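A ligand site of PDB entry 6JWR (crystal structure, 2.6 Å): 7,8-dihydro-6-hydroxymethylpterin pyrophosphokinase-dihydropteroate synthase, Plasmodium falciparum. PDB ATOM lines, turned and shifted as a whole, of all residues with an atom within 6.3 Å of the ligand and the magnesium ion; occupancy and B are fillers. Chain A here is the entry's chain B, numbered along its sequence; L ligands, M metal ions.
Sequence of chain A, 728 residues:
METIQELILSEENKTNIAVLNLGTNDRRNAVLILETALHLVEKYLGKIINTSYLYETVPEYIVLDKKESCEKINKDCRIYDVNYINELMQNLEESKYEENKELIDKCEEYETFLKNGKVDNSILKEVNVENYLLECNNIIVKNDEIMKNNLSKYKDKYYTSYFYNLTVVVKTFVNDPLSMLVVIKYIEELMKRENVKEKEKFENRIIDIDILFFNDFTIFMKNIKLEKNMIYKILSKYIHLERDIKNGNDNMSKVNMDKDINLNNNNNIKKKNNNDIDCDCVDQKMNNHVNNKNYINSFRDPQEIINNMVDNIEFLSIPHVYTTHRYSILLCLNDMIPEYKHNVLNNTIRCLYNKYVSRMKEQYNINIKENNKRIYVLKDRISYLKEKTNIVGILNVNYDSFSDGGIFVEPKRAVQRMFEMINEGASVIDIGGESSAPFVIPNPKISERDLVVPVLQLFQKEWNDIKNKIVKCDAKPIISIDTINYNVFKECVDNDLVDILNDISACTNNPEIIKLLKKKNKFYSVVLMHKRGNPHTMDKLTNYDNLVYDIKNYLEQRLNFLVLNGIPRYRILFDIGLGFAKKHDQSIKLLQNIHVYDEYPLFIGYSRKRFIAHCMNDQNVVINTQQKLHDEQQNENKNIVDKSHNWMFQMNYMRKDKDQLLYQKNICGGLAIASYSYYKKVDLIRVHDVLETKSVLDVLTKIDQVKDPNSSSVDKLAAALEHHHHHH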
ATOM      1  N   LEU A 181       8.166   6.826  10.772  1.00  0.00           N
ATOM      2  CA  LEU A 181       8.334   7.359  12.132  1.00  0.00           C
ATOM      3  C   LEU A 181       9.674   8.072  12.354  1.00  0.00           C
ATOM      4  O   LEU A 181       9.753   9.062  13.084  1.00  0.00           O
ATOM      5  CB  LEU A 181       8.117   6.256  13.186  1.00  0.00           C
ATOM      6  CG  LEU A 181       8.089   6.569  14.708  1.00  0.00           C
ATOM      7  CD1 LEU A 181       7.116   7.678  15.095  1.00  0.00           C
ATOM      8  CD2 LEU A 181       7.784   5.312  15.508  1.00  0.00           C
ATOM      9  N   ILE A 184       9.348  11.292  10.354  1.00  0.00           N
ATOM     10  CA  ILE A 184       8.333  11.993  11.136  1.00  0.00           C
ATOM     11  C   ILE A 184       8.912  12.702  12.365  1.00  0.00           C
ATOM     12  O   ILE A 184       8.660  13.897  12.569  1.00  0.00           O
ATOM     13  CB  ILE A 184       7.155  11.052  11.507  1.00  0.00           C
ATOM     14  CG1 ILE A 184       6.177  10.951  10.327  1.00  0.00           C
ATOM     15  CG2 ILE A 184       6.442  11.496  12.784  1.00  0.00           C
ATOM     16  CD1 ILE A 184       5.168   9.845  10.456  1.00  0.00           C
ATOM     17  N   LYS A 185       9.686  11.959  13.176  1.00  0.00           N
ATOM     18  CA  LYS A 185      10.327  12.525  14.378  1.00  0.00           C
ATOM     19  C   LYS A 185      11.433  13.503  13.991  1.00  0.00           C
ATOM     20  O   LYS A 185      11.764  14.402  14.780  1.00  0.00           O
ATOM     21  CB  LYS A 185      10.874  11.432  15.308  1.00  0.00           C
ATOM     22  CG  LYS A 185       9.823  10.555  15.975  1.00  0.00           C
ATOM     23  CD  LYS A 185       9.023  11.264  17.052  1.00  0.00           C
ATOM     24  CE  LYS A 185       8.026  10.286  17.663  1.00  0.00           C
ATOM     25  NZ  LYS A 185       6.724  10.932  18.000  1.00  0.00           N
ATOM     26  N   GLU A 188       9.104  16.401  13.158  1.00  0.00           N
ATOM     27  CA  GLU A 188       8.742  16.856  14.516  1.00  0.00           C
ATOM     28  C   GLU A 188       9.803  17.777  15.114  1.00  0.00           C
ATOM     29  O   GLU A 188       9.508  18.908  15.509  1.00  0.00           O
ATOM     30  CB  GLU A 188       8.465  15.677  15.464  1.00  0.00           C
ATOM     31  CG  GLU A 188       7.050  15.126  15.405  1.00  0.00           C
ATOM     32  CD  GLU A 188       6.640  14.342  16.657  1.00  0.00           C
ATOM     33  OE1 GLU A 188       6.690  14.903  17.779  1.00  0.00           O
ATOM     34  OE2 GLU A 188       6.243  13.163  16.519  1.00  0.00           O
ATOM     35  N   ASP A 208       2.692  16.872  17.209  1.00  0.00           N
ATOM     36  CA  ASP A 208       2.769  15.421  17.382  1.00  0.00           C
ATOM     37  C   ASP A 208       2.179  14.682  16.164  1.00  0.00           C
ATOM     38  O   ASP A 208       0.957  14.619  15.982  1.00  0.00           O
ATOM     39  CB  ASP A 208       2.111  14.981  18.718  1.00  0.00           C
ATOM     40  CG  ASP A 208       2.276  13.479  19.012  1.00  0.00           C
ATOM     41  OD1 ASP A 208       3.368  12.897  18.785  1.00  0.00           O
ATOM     42  OD2 ASP A 208       1.313  12.875  19.515  1.00  0.00           O
ATOM     43  N   ILE A 209       3.079  14.141  15.330  1.00  0.00           N
ATOM     44  CA  ILE A 209       2.679  13.342  14.163  1.00  0.00           C
ATOM     45  C   ILE A 209       2.756  11.859  14.510  1.00  0.00           C
ATOM     46  O   ILE A 209       3.806  11.355  14.881  1.00  0.00           O
ATOM     47  CB  ILE A 209       3.499  13.639  12.891  1.00  0.00           C
ATOM     48  CG1 ILE A 209       3.624  15.140  12.640  1.00  0.00           C
ATOM     49  CG2 ILE A 209       2.894  12.927  11.685  1.00  0.00           C
ATOM     50  CD1 ILE A 209       4.771  15.519  11.729  1.00  0.00           C
ATOM     51  N   ASP A 210       1.617  11.192  14.383  1.00  0.00           N
ATOM     52  CA  ASP A 210       1.522   9.772  14.653  1.00  0.00           C
ATOM     53  C   ASP A 210       1.142   9.026  13.384  1.00  0.00           C
ATOM     54  O   ASP A 210       0.710   9.640  12.412  1.00  0.00           O
ATOM     55  CB  ASP A 210       0.482   9.521  15.749  1.00  0.00           C
ATOM     56  CG  ASP A 210       0.769  10.308  17.003  1.00  0.00           C
ATOM     57  OD1 ASP A 210       0.766  11.560  16.935  1.00  0.00           O
ATOM     58  OD2 ASP A 210       0.994   9.680  18.061  1.00  0.00           O
ATOM     59  N   ILE A 211       1.350   7.710  13.398  1.00  0.00           N
ATOM     60  CA  ILE A 211       0.905   6.848  12.306  1.00  0.00           C
ATOM     61  C   ILE A 211      -0.190   5.988  12.896  1.00  0.00           C
ATOM     62  O   ILE A 211       0.000   5.329  13.901  1.00  0.00           O
ATOM     63  CB  ILE A 211       2.058   5.971  11.740  1.00  0.00           C
ATOM     64  CG1 ILE A 211       3.281   6.845  11.421  1.00  0.00           C
ATOM     65  CG2 ILE A 211       1.590   5.230  10.493  1.00  0.00           C
ATOM     66  CD1 ILE A 211       4.621   6.171  11.683  1.00  0.00           C
ATOM     67  N   LEU A 212      -1.354   6.017  12.245  1.00  0.00           N
ATOM     68  CA  LEU A 212      -2.538   5.329  12.755  1.00  0.00           C
ATOM     69  C   LEU A 212      -2.763   3.991  12.070  1.00  0.00           C
ATOM     70  O   LEU A 212      -3.248   3.047  12.692  1.00  0.00           O
ATOM     71  CB  LEU A 212      -3.782   6.236  12.644  1.00  0.00           C
ATOM     72  CG  LEU A 212      -3.685   7.701  13.134  1.00  0.00           C
ATOM     73  CD1 LEU A 212      -4.783   8.545  12.502  1.00  0.00           C
ATOM     74  CD2 LEU A 212      -3.696   7.831  14.653  1.00  0.00           C
ATOM     75  N   ASN A 312      14.139   9.763  21.861  1.00  0.00           N
ATOM     76  CA  ASN A 312      12.736  10.111  21.593  1.00  0.00           C
ATOM     77  C   ASN A 312      11.906   8.955  21.028  1.00  0.00           C
ATOM     78  O   ASN A 312      10.826   8.667  21.558  1.00  0.00           O
ATOM     79  CB  ASN A 312      12.626  11.352  20.682  1.00  0.00           C
ATOM     80  CG  ASN A 312      12.968  12.665  21.402  1.00  0.00           C
ATOM     81  OD1 ASN A 312      12.816  12.787  22.623  1.00  0.00           O
ATOM     82  ND2 ASN A 312      13.415  13.643  20.633  1.00  0.00           N
ATOM     83  N   ILE A 313      12.413   8.296  19.989  1.00  0.00           N
ATOM     84  CA  ILE A 313      11.770   7.086  19.439  1.00  0.00           C
ATOM     85  C   ILE A 313      12.048   5.932  20.395  1.00  0.00           C
ATOM     86  O   ILE A 313      13.205   5.687  20.781  1.00  0.00           O
ATOM     87  CB  ILE A 313      12.216   6.733  17.997  1.00  0.00           C
ATOM     88  CG1 ILE A 313      12.256   7.981  17.102  1.00  0.00           C
ATOM     89  CG2 ILE A 313      11.293   5.669  17.398  1.00  0.00           C
ATOM     90  CD1 ILE A 313      13.170   7.874  15.895  1.00  0.00           C
ATOM     91  N   GLU A 314      10.981   5.228  20.773  1.00  0.00           N
ATOM     92  CA  GLU A 314      11.069   4.183  21.789  1.00  0.00           C
ATOM     93  C   GLU A 314      10.428   2.873  21.308  1.00  0.00           C
ATOM     94  O   GLU A 314      11.002   1.801  21.509  1.00  0.00           O
ATOM     95  CB  GLU A 314      10.479   4.673  23.135  1.00  0.00           C
ATOM     96  CG  GLU A 314      11.184   5.916  23.716  1.00  0.00           C
ATOM     97  CD  GLU A 314      10.872   6.203  25.181  1.00  0.00           C
ATOM     98  OE1 GLU A 314       9.687   6.149  25.593  1.00  0.00           O
ATOM     99  OE2 GLU A 314      11.824   6.529  25.933  1.00  0.00           O
ATOM    100  N   PHE A 315       9.253   2.964  20.678  1.00  0.00           N
ATOM    101  CA  PHE A 315       8.564   1.787  20.095  1.00  0.00           C
ATOM    102  C   PHE A 315       7.706   2.131  18.854  1.00  0.00           C
ATOM    103  O   PHE A 315       7.750   3.266  18.356  1.00  0.00           O
ATOM    104  CB  PHE A 315       7.793   0.985  21.185  1.00  0.00           C
ATOM    105  CG  PHE A 315       6.482   1.593  21.613  1.00  0.00           C
ATOM    106  CD1 PHE A 315       6.425   2.849  22.254  1.00  0.00           C
ATOM    107  CD2 PHE A 315       5.291   0.895  21.414  1.00  0.00           C
ATOM    108  CE1 PHE A 315       5.210   3.388  22.653  1.00  0.00           C
ATOM    109  CE2 PHE A 315       4.072   1.434  21.826  1.00  0.00           C
ATOM    110  CZ  PHE A 315       4.024   2.676  22.440  1.00  0.00           C
ATOM    111  N   LEU A 316       6.951   1.138  18.343  1.00  0.00           N
ATOM    112  CA  LEU A 316       6.030   1.318  17.211  1.00  0.00           C
ATOM    113  C   LEU A 316       4.814   0.358  17.243  1.00  0.00           C
ATOM    114  O   LEU A 316       4.978  -0.863  17.278  1.00  0.00           O
ATOM    115  CB  LEU A 316       6.780   1.227  15.862  1.00  0.00           C
ATOM    116  CG  LEU A 316       6.002   1.367  14.545  1.00  0.00           C
ATOM    117  CD1 LEU A 316       6.598   2.433  13.642  1.00  0.00           C
ATOM    118  CD2 LEU A 316       5.931   0.030  13.825  1.00  0.00           C
ATOM    119  N   SER A 317       3.612   0.940  17.245  1.00  0.00           N
ATOM    120  CA  SER A 317       2.369   0.171  17.155  1.00  0.00           C
ATOM    121  C   SER A 317       1.483   0.640  15.984  1.00  0.00           C
ATOM    122  O   SER A 317       1.133   1.823  15.879  1.00  0.00           O
ATOM    123  CB  SER A 317       1.580   0.210  18.470  1.00  0.00           C
ATOM    124  OG  SER A 317       0.438  -0.657  18.422  1.00  0.00           O
ATOM    125  N   ILE A 318       1.154  -0.315  15.121  1.00  0.00           N
ATOM    126  CA  ILE A 318       0.239  -0.134  14.005  1.00  0.00           C
ATOM    127  C   ILE A 318      -0.870  -1.193  14.140  1.00  0.00           C
ATOM    128  O   ILE A 318      -0.560  -2.393  14.161  1.00  0.00           O
ATOM    129  CB  ILE A 318       1.025  -0.151  12.653  1.00  0.00           C
ATOM    130  CG1 ILE A 318       1.394   1.283  12.233  1.00  0.00           C
ATOM    131  CG2 ILE A 318       0.216  -0.798  11.530  1.00  0.00           C
ATOM    132  CD1 ILE A 318       2.666   1.827  12.825  1.00  0.00           C
ATOM    133  N   PRO A 319      -2.145  -0.790  14.292  1.00  0.00           N
ATOM    134  CA  PRO A 319      -2.575   0.602  14.474  1.00  0.00           C
ATOM    135  C   PRO A 319      -2.031   1.264  15.737  1.00  0.00           C
ATOM    136  O   PRO A 319      -1.656   0.552  16.683  1.00  0.00           O
ATOM    137  CB  PRO A 319      -4.108   0.477  14.564  1.00  0.00           C
ATOM    138  CG  PRO A 319      -4.460  -0.936  14.208  1.00  0.00           C
ATOM    139  CD  PRO A 319      -3.216  -1.598  13.696  1.00  0.00           C
ATOM    140  N   HIS A 320      -1.991   2.603  15.756  1.00  0.00           N
ATOM    141  CA  HIS A 320      -1.626   3.399  16.943  1.00  0.00           C
ATOM    142  C   HIS A 320      -2.452   2.960  18.164  1.00  0.00           C
ATOM    143  O   HIS A 320      -3.598   2.535  18.016  1.00  0.00           O
ATOM    144  CB  HIS A 320      -1.808   4.892  16.680  1.00  0.00           C
ATOM    145  CG  HIS A 320      -1.136   5.777  17.684  1.00  0.00           C
ATOM    146  ND1 HIS A 320      -1.699   6.080  18.906  1.00  0.00           N
ATOM    147  CD2 HIS A 320       0.039   6.457  17.623  1.00  0.00           C
ATOM    148  CE1 HIS A 320      -0.892   6.899  19.561  1.00  0.00           C
ATOM    149  NE2 HIS A 320       0.165   7.139  18.812  1.00  0.00           N
ATOM    150  N   VAL A 321      -1.845   3.055  19.339  1.00  0.00           N
ATOM    151  CA  VAL A 321      -2.417   2.511  20.575  1.00  0.00           C
ATOM    152  C   VAL A 321      -3.817   3.070  20.921  1.00  0.00           C
ATOM    153  O   VAL A 321      -4.780   2.294  21.075  1.00  0.00           O
ATOM    154  CB  VAL A 321      -1.418   2.536  21.779  1.00  0.00           C
ATOM    155  CG1 VAL A 321      -0.489   1.332  21.727  1.00  0.00           C
ATOM    156  CG2 VAL A 321      -0.606   3.826  21.834  1.00  0.00           C
ATOM    157  N   TYR A 322      -3.923   4.394  20.992  1.00  0.00           N
ATOM    158  CA  TYR A 322      -5.149   5.073  21.466  1.00  0.00           C
ATOM    159  C   TYR A 322      -6.292   5.160  20.421  1.00  0.00           C
ATOM    160  O   TYR A 322      -7.415   5.567  20.749  1.00  0.00           O
ATOM    161  CB  TYR A 322      -4.830   6.487  21.995  1.00  0.00           C
ATOM    162  CG  TYR A 322      -3.667   6.602  22.966  1.00  0.00           C
ATOM    163  CD1 TYR A 322      -3.758   6.110  24.287  1.00  0.00           C
ATOM    164  CD2 TYR A 322      -2.484   7.266  22.593  1.00  0.00           C
ATOM    165  CE1 TYR A 322      -2.700   6.237  25.181  1.00  0.00           C
ATOM    166  CE2 TYR A 322      -1.415   7.410  23.476  1.00  0.00           C
ATOM    167  CZ  TYR A 322      -1.527   6.894  24.769  1.00  0.00           C
ATOM    168  OH  TYR A 322      -0.467   7.044  25.643  1.00  0.00           O
ATOM    169  N   ARG A 326      -9.396   7.041  22.133  1.00  0.00           N
ATOM    170  CA  ARG A 326      -9.497   8.511  22.006  1.00  0.00           C
ATOM    171  C   ARG A 326     -10.646   8.923  21.075  1.00  0.00           C
ATOM    172  O   ARG A 326     -10.763   8.412  19.953  1.00  0.00           O
ATOM    173  CB  ARG A 326      -8.172   9.134  21.535  1.00  0.00           C
ATOM    174  CG  ARG A 326      -7.182   9.394  22.651  1.00  0.00           C
ATOM    175  CD  ARG A 326      -5.905  10.062  22.149  1.00  0.00           C
ATOM    176  NE  ARG A 326      -5.246  10.832  23.203  1.00  0.00           N
ATOM    177  CZ  ARG A 326      -3.921  11.019  23.298  1.00  0.00           C
ATOM    178  NH1 ARG A 326      -3.082  10.495  22.413  1.00  0.00           N
ATOM    179  NH2 ARG A 326      -3.433  11.744  24.308  1.00  0.00           N
HETATM  180  P1  LIG L   1       3.072  10.547  22.168  1.00  0.00           P
HETATM  181  O1  LIG L   1       3.109  10.511  23.678  1.00  0.00           O
HETATM  182  O2  LIG L   1       3.430  11.911  21.612  1.00  0.00           O
HETATM  183  O3  LIG L   1       1.842   9.886  21.575  1.00  0.00           O
HETATM  184  O4  LIG L   1       4.341   9.644  21.725  1.00  0.00           O
HETATM  185  C1  LIG L   1       4.252   8.223  21.639  1.00  0.00           C
HETATM  186  C2  LIG L   1       5.616   7.567  21.433  1.00  0.00           C
HETATM  187  O5  LIG L   1       5.406   6.181  21.158  1.00  0.00           O
HETATM  188  C3  LIG L   1       6.438   8.125  20.267  1.00  0.00           C
HETATM  189  O6  LIG L   1       7.585   8.844  20.718  1.00  0.00           O
HETATM  190  C4  LIG L   1       6.854   6.936  19.411  1.00  0.00           C
HETATM  191  O7  LIG L   1       8.261   6.677  19.465  1.00  0.00           O
HETATM  192  C5  LIG L   1       6.057   5.750  19.961  1.00  0.00           C
HETATM  193  N1  LIG L   1       5.025   5.192  19.034  1.00  0.00           N
HETATM  194  C6  LIG L   1       4.510   3.941  19.184  1.00  0.00           C
HETATM  195  N2  LIG L   1       3.584   3.642  18.243  1.00  0.00           N
HETATM  196  C7  LIG L   1       3.479   4.718  17.451  1.00  0.00           C
HETATM  197  C8  LIG L   1       2.670   5.073  16.259  1.00  0.00           C
HETATM  198  N3  LIG L   1       1.784   4.196  15.734  1.00  0.00           N
HETATM  199  N4  LIG L   1       2.849   6.314  15.718  1.00  0.00           N
HETATM  200  C9  LIG L   1       3.725   7.212  16.234  1.00  0.00           C
HETATM  201  N5  LIG L   1       4.491   6.953  17.317  1.00  0.00           N
HETATM  202  C10 LIG L   1       4.416   5.742  17.965  1.00  0.00           C
HETATM  203 MG    MG M   1       1.973  10.333  19.781  1.00  0.00          MG
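The backbone NH of Ser 317 lies within hydrogen-bond range of a nitrogen (N2) of the ligand (2.9 Å). O of Ser 317 lies within hydrogen-bond range of N3 of the ligand (2.5 Å). OD1 of Asp 208 lies close to O2 of the ligand (3.0 Å). N of Ile 211 sits at hydrogen-bond distance from N4 of the ligand. A nitrogen (N3) of the ligand sits at hydrogen-bond distance from the backbone carbonyl oxygen (O) of Ile 211, 2.8 Å away. N of Glu 314 is in hydrogen-bond range of O7 of the ligand (3.3 Å). O6 of the ligand lies within hydrogen-bond range of O of Asn 312 (3.4 Å).
The side-chain carboxylate of Asp 210 sits close to a ring nitrogen (NE2) of His 320 (2.8 Å). O of Pro 319 is in hydrogen-bond range of OG of Ser 317, at 3.0 Å. NZ of Lys 185 lies within salt-bridge range of OD1 of Asp 208. A ring nitrogen (ND1) of His 320 is in hydrogen-bond range of the backbone NH of Tyr 322 (3.5 Å). The backbone carbonyl oxygen (O) of Leu 212 is in hydrogen-bond range of the backbone NH (N) of His 320 (3.3 Å). The side-chain amino group (NZ) of Lys 185 is in salt-bridge range of the side-chain carboxylate (OE2) of Glu 188 (2.7 Å).
A nitrogen (N1) of the ligand sits close to the backbone carbonyl oxygen (O) of Phe 315 (3.4 Å). Leu 181 touches the ligand (CD1 to N5, 3.5 Å). Lys 185 touches the ligand. CA of Ile 313 touches O7 of the ligand, at 3.5 Å. Leu 316 touches the ligand. CD1 of Ile 318 touches N3 of the ligand, at 3.9 Å. His 320 touches the ligand (CD2 to C8, 3.3 Å). Within 4 Å of the ligand: Leu 181, Lys 185, Asp 208, Asp 210, Ile 211, Asn 312, Ile 313, Glu 314, Phe 315, Leu 316, Ser 317, Ile 318 and His 320. Along chain A the residues within 4 Å of the ligand span positions 181 to 320. The nearest printed residue that does not touch the ligand is Ile 209 (4.4 Å).
Residues that only touch the magnesium ion: His 320 (3.8 Å). Of the 21 residues printed, 3 come within 4 Å of the magnesium ion.
The magnesium ion is bound by an oxygen (O3) of the ligand and the side-chain carboxylate (OD2) of Asp 210. The magnesium ion has two donor atoms within binding distance. Slightly farther from the magnesium ion lies OD2 of Asp 208 (2.6 Å). Slightly farther from the magnesium ion lies an oxygen (O2) of the ligand (2.8 Å).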
